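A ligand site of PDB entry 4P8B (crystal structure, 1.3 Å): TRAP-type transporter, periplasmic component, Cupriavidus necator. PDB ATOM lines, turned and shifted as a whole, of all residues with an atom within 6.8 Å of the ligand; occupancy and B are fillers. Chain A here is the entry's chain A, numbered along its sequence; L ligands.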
ATOM      1  N   VAL A  38      14.531  13.760 -24.221  1.00  0.00           N
ATOM      2  CA  VAL A  38      15.291  14.591 -23.309  1.00  0.00           C
ATOM      3  C   VAL A  38      14.440  14.916 -22.086  1.00  0.00           C
ATOM      4  O   VAL A  38      14.900  14.778 -20.962  1.00  0.00           O
ATOM      5  CB  VAL A  38      15.758  15.898 -23.960  1.00  0.00           C
ATOM      6  CG1 VAL A  38      16.438  16.798 -22.948  1.00  0.00           C
ATOM      7  CG2 VAL A  38      16.701  15.620 -25.086  1.00  0.00           C
ATOM      8  N   LEU A  39      13.200  15.320 -22.317  1.00  0.00           N
ATOM      9  CA  LEU A  39      12.277  15.727 -21.249  1.00  0.00           C
ATOM     10  C   LEU A  39      11.207  14.679 -20.994  1.00  0.00           C
ATOM     11  O   LEU A  39      10.638  14.116 -21.934  1.00  0.00           O
ATOM     12  CB  LEU A  39      11.585  17.031 -21.655  1.00  0.00           C
ATOM     13  CG  LEU A  39      12.521  18.226 -21.893  1.00  0.00           C
ATOM     14  CD1 LEU A  39      11.702  19.482 -22.204  1.00  0.00           C
ATOM     15  CD2 LEU A  39      13.427  18.451 -20.677  1.00  0.00           C
ATOM     16  N   TRP A  45       6.669  17.949 -24.103  1.00  0.00           N
ATOM     17  CA  TRP A  45       7.481  17.068 -24.957  1.00  0.00           C
ATOM     18  C   TRP A  45       7.348  15.614 -24.491  1.00  0.00           C
ATOM     19  O   TRP A  45       6.998  14.717 -25.285  1.00  0.00           O
ATOM     20  CB  TRP A  45       8.920  17.559 -24.877  1.00  0.00           C
ATOM     21  CG  TRP A  45      10.005  16.788 -25.551  1.00  0.00           C
ATOM     22  CD1 TRP A  45      10.000  15.498 -26.012  1.00  0.00           C
ATOM     23  CD2 TRP A  45      11.285  17.326 -25.841  1.00  0.00           C
ATOM     24  NE1 TRP A  45      11.233  15.200 -26.530  1.00  0.00           N
ATOM     25  CE2 TRP A  45      12.041  16.306 -26.450  1.00  0.00           C
ATOM     26  CE3 TRP A  45      11.874  18.571 -25.626  1.00  0.00           C
ATOM     27  CZ2 TRP A  45      13.356  16.501 -26.851  1.00  0.00           C
ATOM     28  CZ3 TRP A  45      13.158  18.771 -26.031  1.00  0.00           C
ATOM     29  CH2 TRP A  45      13.907  17.725 -26.621  1.00  0.00           C
ATOM     30  N   GLN A  79      22.621  14.779 -25.332  1.00  0.00           N
ATOM     31  CA  GLN A  79      21.530  14.887 -26.272  1.00  0.00           C
ATOM     32  C   GLN A  79      21.986  15.261 -27.682  1.00  0.00           C
ATOM     33  O   GLN A  79      21.264  14.994 -28.654  1.00  0.00           O
ATOM     34  CB  GLN A  79      20.502  15.897 -25.742  1.00  0.00           C
ATOM     35  CG  GLN A  79      21.032  17.338 -25.636  1.00  0.00           C
ATOM     36  CD  GLN A  79      20.259  18.155 -24.648  1.00  0.00           C
ATOM     37  OE1 GLN A  79      20.285  17.861 -23.476  1.00  0.00           O
ATOM     38  NE2 GLN A  79      19.576  19.177 -25.128  1.00  0.00           N
ATOM     39  N   SER A  97      14.125  17.125 -30.333  1.00  0.00           N
ATOM     40  CA  SER A  97      14.185  18.517 -30.759  1.00  0.00           C
ATOM     41  C   SER A  97      15.119  18.667 -31.942  1.00  0.00           C
ATOM     42  O   SER A  97      16.217  18.102 -31.985  1.00  0.00           O
ATOM     43  CB  SER A  97      14.697  19.411 -29.639  1.00  0.00           C
ATOM     44  OG  SER A  97      14.998  20.706 -30.173  1.00  0.00           O
ATOM     45  N   THR A  98      14.702  19.489 -32.900  1.00  0.00           N
ATOM     46  CA  THR A  98      15.536  19.804 -34.045  1.00  0.00           C
ATOM     47  C   THR A  98      16.904  20.368 -33.636  1.00  0.00           C
ATOM     48  O   THR A  98      17.885  20.192 -34.365  1.00  0.00           O
ATOM     49  CB  THR A  98      14.822  20.746 -35.020  1.00  0.00           C
ATOM     50  OG1 THR A  98      14.454  21.945 -34.334  1.00  0.00           O
ATOM     51  CG2 THR A  98      13.575  20.076 -35.601  1.00  0.00           C
ATOM     52  N   ILE A  99      16.981  21.052 -32.495  1.00  0.00           N
ATOM     53  CA  ILE A  99      18.234  21.610 -32.050  1.00  0.00           C
ATOM     54  C   ILE A  99      19.264  20.492 -31.793  1.00  0.00           C
ATOM     55  O   ILE A  99      20.423  20.574 -32.179  1.00  0.00           O
ATOM     56  CB  ILE A  99      18.051  22.451 -30.778  1.00  0.00           C
ATOM     57  CG1 ILE A  99      17.278  23.726 -31.119  1.00  0.00           C
ATOM     58  CG2 ILE A  99      19.419  22.800 -30.179  1.00  0.00           C
ATOM     59  CD1 ILE A  99      16.888  24.529 -29.895  1.00  0.00           C
ATOM     60  N   ASN A 100      18.810  19.427 -31.151  1.00  0.00           N
ATOM     61  CA  ASN A 100      19.733  18.391 -30.691  1.00  0.00           C
ATOM     62  C   ASN A 100      20.288  17.552 -31.815  1.00  0.00           C
ATOM     63  O   ASN A 100      21.386  17.004 -31.696  1.00  0.00           O
ATOM     64  CB  ASN A 100      19.038  17.497 -29.686  1.00  0.00           C
ATOM     65  CG  ASN A 100      18.709  18.227 -28.400  1.00  0.00           C
ATOM     66  OD1 ASN A 100      19.364  19.210 -28.039  1.00  0.00           O
ATOM     67  ND2 ASN A 100      17.631  17.820 -27.766  1.00  0.00           N
ATOM     68  N   ASN A 152       8.446  22.079 -29.073  1.00  0.00           N
ATOM     69  CA  ASN A 152       8.969  22.559 -27.798  1.00  0.00           C
ATOM     70  C   ASN A 152       8.465  23.995 -27.656  1.00  0.00           C
ATOM     71  O   ASN A 152       7.631  24.255 -26.786  1.00  0.00           O
ATOM     72  CB  ASN A 152      10.489  22.424 -27.771  1.00  0.00           C
ATOM     73  CG  ASN A 152      11.047  22.166 -26.375  1.00  0.00           C
ATOM     74  OD1 ASN A 152      10.319  21.841 -25.429  1.00  0.00           O
ATOM     75  ND2 ASN A 152      12.351  22.286 -26.251  1.00  0.00           N
ATOM     76  N   ARG A 155      11.731  30.064 -27.901  1.00  0.00           N
ATOM     77  CA  ARG A 155      12.718  29.956 -26.833  1.00  0.00           C
ATOM     78  C   ARG A 155      13.043  31.345 -26.283  1.00  0.00           C
ATOM     79  O   ARG A 155      13.719  32.136 -26.910  1.00  0.00           O
ATOM     80  CB  ARG A 155      13.972  29.230 -27.347  1.00  0.00           C
ATOM     81  CG  ARG A 155      13.659  27.838 -27.876  1.00  0.00           C
ATOM     82  CD  ARG A 155      14.884  27.111 -28.387  1.00  0.00           C
ATOM     83  NE  ARG A 155      15.845  26.742 -27.333  1.00  0.00           N
ATOM     84  CZ  ARG A 155      15.806  25.637 -26.607  1.00  0.00           C
ATOM     85  NH1 ARG A 155      14.814  24.787 -26.731  1.00  0.00           N
ATOM     86  NH2 ARG A 155      16.754  25.409 -25.711  1.00  0.00           N
ATOM     87  N   ARG A 176      23.697  29.828 -20.881  1.00  0.00           N
ATOM     88  CA  ARG A 176      23.752  28.465 -21.367  1.00  0.00           C
ATOM     89  C   ARG A 176      22.975  28.328 -22.662  1.00  0.00           C
ATOM     90  O   ARG A 176      21.858  28.826 -22.779  1.00  0.00           O
ATOM     91  CB  ARG A 176      23.196  27.513 -20.312  1.00  0.00           C
ATOM     92  CG  ARG A 176      23.140  26.040 -20.738  1.00  0.00           C
ATOM     93  CD  ARG A 176      21.807  25.746 -21.365  1.00  0.00           C
ATOM     94  NE  ARG A 176      21.725  24.360 -21.823  1.00  0.00           N
ATOM     95  CZ  ARG A 176      20.618  23.816 -22.318  1.00  0.00           C
ATOM     96  NH1 ARG A 176      19.498  24.518 -22.407  1.00  0.00           N
ATOM     97  NH2 ARG A 176      20.632  22.545 -22.704  1.00  0.00           N
ATOM     98  N   VAL A 177      23.561  27.575 -23.601  1.00  0.00           N
ATOM     99  CA  VAL A 177      22.903  27.147 -24.817  1.00  0.00           C
ATOM    100  C   VAL A 177      23.143  25.638 -24.986  1.00  0.00           C
ATOM    101  O   VAL A 177      23.992  25.061 -24.299  1.00  0.00           O
ATOM    102  CB  VAL A 177      23.398  27.947 -26.064  1.00  0.00           C
ATOM    103  CG1 VAL A 177      23.034  29.440 -25.913  1.00  0.00           C
ATOM    104  CG2 VAL A 177      24.877  27.752 -26.290  1.00  0.00           C
ATOM    105  N   VAL A 178      22.426  25.014 -25.913  1.00  0.00           N
ATOM    106  CA  VAL A 178      22.700  23.629 -26.271  1.00  0.00           C
ATOM    107  C   VAL A 178      23.942  23.626 -27.123  1.00  0.00           C
ATOM    108  O   VAL A 178      24.233  24.636 -27.794  1.00  0.00           O
ATOM    109  CB  VAL A 178      21.513  23.059 -27.076  1.00  0.00           C
ATOM    110  CG1 VAL A 178      21.816  21.641 -27.527  1.00  0.00           C
ATOM    111  CG2 VAL A 178      20.247  23.101 -26.241  1.00  0.00           C
ATOM    112  N   MET A 197      25.997  23.335 -23.018  1.00  0.00           N
ATOM    113  CA  MET A 197      25.891  22.132 -22.205  1.00  0.00           C
ATOM    114  C   MET A 197      24.522  21.496 -22.314  1.00  0.00           C
ATOM    115  O   MET A 197      23.563  22.127 -22.744  1.00  0.00           O
ATOM    116  CB  MET A 197      26.220  22.430 -20.748  1.00  0.00           C
ATOM    117  CG  MET A 197      25.204  23.275 -20.080  1.00  0.00           C
ATOM    118  SD  MET A 197      25.813  24.063 -18.387  1.00  0.00           S
ATOM    119  CE  MET A 197      27.019  25.352 -19.097  1.00  0.00           C
ATOM    120  N   SER A 198      24.476  20.210 -21.999  1.00  0.00           N
ATOM    121  CA  SER A 198      23.231  19.448 -22.033  1.00  0.00           C
ATOM    122  C   SER A 198      22.209  20.005 -21.076  1.00  0.00           C
ATOM    123  O   SER A 198      22.519  20.755 -20.146  1.00  0.00           O
ATOM    124  CB  SER A 198      23.489  18.005 -21.653  1.00  0.00           C
ATOM    125  OG  SER A 198      23.859  17.936 -20.276  1.00  0.00           O
ATOM    126  N   TRP A 199      20.953  19.619 -21.280  1.00  0.00           N
ATOM    127  CA  TRP A 199      19.886  20.007 -20.392  1.00  0.00           C
ATOM    128  C   TRP A 199      20.203  19.536 -18.956  1.00  0.00           C
ATOM    129  O   TRP A 199      20.023  20.282 -17.994  1.00  0.00           O
ATOM    130  CB  TRP A 199      18.559  19.419 -20.875  1.00  0.00           C
ATOM    131  CG  TRP A 199      17.429  19.574 -19.901  1.00  0.00           C
ATOM    132  CD1 TRP A 199      16.829  18.575 -19.201  1.00  0.00           C
ATOM    133  CD2 TRP A 199      16.813  20.785 -19.496  1.00  0.00           C
ATOM    134  NE1 TRP A 199      15.848  19.098 -18.402  1.00  0.00           N
ATOM    135  CE2 TRP A 199      15.822  20.461 -18.561  1.00  0.00           C
ATOM    136  CE3 TRP A 199      17.007  22.126 -19.830  1.00  0.00           C
ATOM    137  CZ2 TRP A 199      14.994  21.417 -17.975  1.00  0.00           C
ATOM    138  CZ3 TRP A 199      16.189  23.090 -19.240  1.00  0.00           C
ATOM    139  CH2 TRP A 199      15.199  22.716 -18.305  1.00  0.00           C
ATOM    140  N   ALA A 200      20.730  18.324 -18.795  1.00  0.00           N
ATOM    141  CA  ALA A 200      21.085  17.856 -17.450  1.00  0.00           C
ATOM    142  C   ALA A 200      22.119  18.802 -16.820  1.00  0.00           C
ATOM    143  O   ALA A 200      22.017  19.205 -15.636  1.00  0.00           O
ATOM    144  CB  ALA A 200      21.632  16.430 -17.490  1.00  0.00           C
ATOM    145  N   ALA A 202      22.821  21.864 -17.476  1.00  0.00           N
ATOM    146  CA  ALA A 202      22.329  23.204 -17.257  1.00  0.00           C
ATOM    147  C   ALA A 202      21.786  23.418 -15.861  1.00  0.00           C
ATOM    148  O   ALA A 202      21.886  24.531 -15.320  1.00  0.00           O
ATOM    149  CB  ALA A 202      21.280  23.542 -18.295  1.00  0.00           C
ATOM    150  N   GLN A 214      19.661  31.318 -19.562  1.00  0.00           N
ATOM    151  CA  GLN A 214      19.381  30.235 -20.480  1.00  0.00           C
ATOM    152  C   GLN A 214      18.268  30.690 -21.434  1.00  0.00           C
ATOM    153  O   GLN A 214      17.851  31.859 -21.379  1.00  0.00           O
ATOM    154  CB  GLN A 214      18.961  28.957 -19.689  1.00  0.00           C
ATOM    155  CG  GLN A 214      17.688  29.088 -18.888  1.00  0.00           C
ATOM    156  CD  GLN A 214      16.427  28.789 -19.667  1.00  0.00           C
ATOM    157  OE1 GLN A 214      16.320  27.704 -20.261  1.00  0.00           O
ATOM    158  NE2 GLN A 214      15.456  29.683 -19.660  1.00  0.00           N
ATOM    159  N   GLU A 215      17.789  29.800 -22.293  1.00  0.00           N
ATOM    160  CA  GLU A 215      16.742  30.131 -23.236  1.00  0.00           C
ATOM    161  C   GLU A 215      15.942  28.880 -23.525  1.00  0.00           C
ATOM    162  O   GLU A 215      16.515  27.820 -23.760  1.00  0.00           O
ATOM    163  CB  GLU A 215      17.348  30.751 -24.521  1.00  0.00           C
ATOM    164  CG  GLU A 215      18.587  30.047 -25.080  1.00  0.00           C
ATOM    165  CD  GLU A 215      18.263  28.797 -25.903  1.00  0.00           C
ATOM    166  OE1 GLU A 215      17.517  28.919 -26.896  1.00  0.00           O
ATOM    167  OE2 GLU A 215      18.769  27.689 -25.561  1.00  0.00           O
ATOM    168  N   ASN A 216      14.628  28.966 -23.455  1.00  0.00           N
ATOM    169  CA  ASN A 216      13.796  27.751 -23.587  1.00  0.00           C
ATOM    170  C   ASN A 216      12.337  28.145 -23.718  1.00  0.00           C
ATOM    171  O   ASN A 216      11.955  29.285 -23.388  1.00  0.00           O
ATOM    172  CB  ASN A 216      13.948  26.843 -22.352  1.00  0.00           C
ATOM    173  CG  ASN A 216      14.743  25.573 -22.626  1.00  0.00           C
ATOM    174  OD1 ASN A 216      14.382  24.788 -23.486  1.00  0.00           O
ATOM    175  ND2 ASN A 216      15.813  25.358 -21.876  1.00  0.00           N
ATOM    176  N   PRO A 217      11.491  27.235 -24.211  1.00  0.00           N
ATOM    177  CA  PRO A 217      10.072  27.554 -24.278  1.00  0.00           C
ATOM    178  C   PRO A 217       9.444  27.796 -22.911  1.00  0.00           C
ATOM    179  O   PRO A 217       9.912  27.287 -21.877  1.00  0.00           O
ATOM    180  CB  PRO A 217       9.480  26.323 -24.985  1.00  0.00           C
ATOM    181  CG  PRO A 217      10.621  25.690 -25.664  1.00  0.00           C
ATOM    182  CD  PRO A 217      11.782  25.898 -24.737  1.00  0.00           C
ATOM    183  N   VAL A 220       8.736  24.712 -20.724  1.00  0.00           N
ATOM    184  CA  VAL A 220       9.938  24.147 -20.117  1.00  0.00           C
ATOM    185  C   VAL A 220      10.339  25.009 -18.928  1.00  0.00           C
ATOM    186  O   VAL A 220      10.573  24.477 -17.839  1.00  0.00           O
ATOM    187  CB  VAL A 220      11.049  24.039 -21.153  1.00  0.00           C
ATOM    188  CG1 VAL A 220      12.341  23.588 -20.525  1.00  0.00           C
ATOM    189  CG2 VAL A 220      10.628  23.084 -22.283  1.00  0.00           C
ATOM    190  N   ASP A 242      11.996  25.659 -31.485  1.00  0.00           N
ATOM    191  CA  ASP A 242      12.324  24.314 -31.885  1.00  0.00           C
ATOM    192  C   ASP A 242      11.069  23.441 -31.937  1.00  0.00           C
ATOM    193  O   ASP A 242      10.412  23.227 -30.894  1.00  0.00           O
ATOM    194  CB  ASP A 242      13.466  23.657 -31.048  1.00  0.00           C
ATOM    195  CG  ASP A 242      13.225  23.613 -29.549  1.00  0.00           C
ATOM    196  OD1 ASP A 242      12.772  24.603 -28.944  1.00  0.00           O
ATOM    197  OD2 ASP A 242      13.623  22.575 -28.938  1.00  0.00           O
HETATM  198  O1  LIG L   1      18.266  21.391 -23.707  1.00  0.00           O
HETATM  199  C1  LIG L   1      17.221  22.119 -23.839  1.00  0.00           C
HETATM  200  O2  LIG L   1      17.234  23.354 -23.558  1.00  0.00           O
HETATM  201  C2  LIG L   1      15.943  21.516 -24.339  1.00  0.00           C
HETATM  202  C3  LIG L   1      15.418  20.573 -23.282  1.00  0.00           C
HETATM  203  O3  LIG L   1      15.046  22.509 -24.760  1.00  0.00           O
HETATM  204  C4  LIG L   1      16.330  20.761 -25.577  1.00  0.00           C
HETATM  205  O4  LIG L   1      16.509  19.545 -25.532  1.00  0.00           O
HETATM  206  C5  LIG L   1      16.530  21.492 -26.858  1.00  0.00           C
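Residues that only touch the ligand: Val 38, Leu 39, Trp 45, Ser 97, Val 178, Trp 199 and Asp 242. Within 4 Å of the ligand: Val 38, Leu 39, Trp 45, Gln 79, Ser 97, Asn 100, Asn 152, Arg 155, Arg 176, Val 178, Trp 199, Asn 216 and Asp 242. The nearest printed residue that does not touch the ligand is Ile 99 (4.3 Å).
The side-chain amide oxygen of Asn 216 lies within hydrogen-bond range of the guanidinium group of Arg 155, at 3.3 Å. ND2 of Asn 216 lies within hydrogen-bond range of OE1 of Gln 214 (2.9 Å). The guanidinium group (NH2) of Arg 176 sits at hydrogen-bond distance from the backbone carbonyl oxygen (O) of Met 197 (3.0 Å). OD1 of Asn 100 is in hydrogen-bond range of NE2 of Gln 79 (2.9 Å). N of Trp 199 is in hydrogen-bond range of OE1 of Gln 79, at 2.9 Å. The backbone NH of Asn 152 is in hydrogen-bond range of the backbone carbonyl oxygen of Asp 242 (2.9 Å). The side-chain carboxylate (OD2) of Asp 242 lies within hydrogen-bond range of the side-chain hydroxyl (OG) of Ser 97, at 2.6 Å. N of Ile 99 lies within hydrogen-bond range of OG of Ser 97, at 3.1 Å.
OD1 of Asn 216 lies within hydrogen-bond range of O3 of the ligand (2.7 Å). NH1 of Arg 176 lies within salt-bridge range of O2 of the ligand. The side-chain amide nitrogen (NE2) of Gln 79 sits at hydrogen-bond distance from an oxygen (O1) of the ligand (2.9 Å). An oxygen (O2) of the ligand is in salt-bridge range of the guanidinium group (NH2) of Arg 155 (3.0 Å). ND2 of Asn 100 is in hydrogen-bond range of O4 of the ligand (3.0 Å). ND2 of Asn 152 sits at hydrogen-bond distance from O3 of the ligand, 3.1 Å away.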
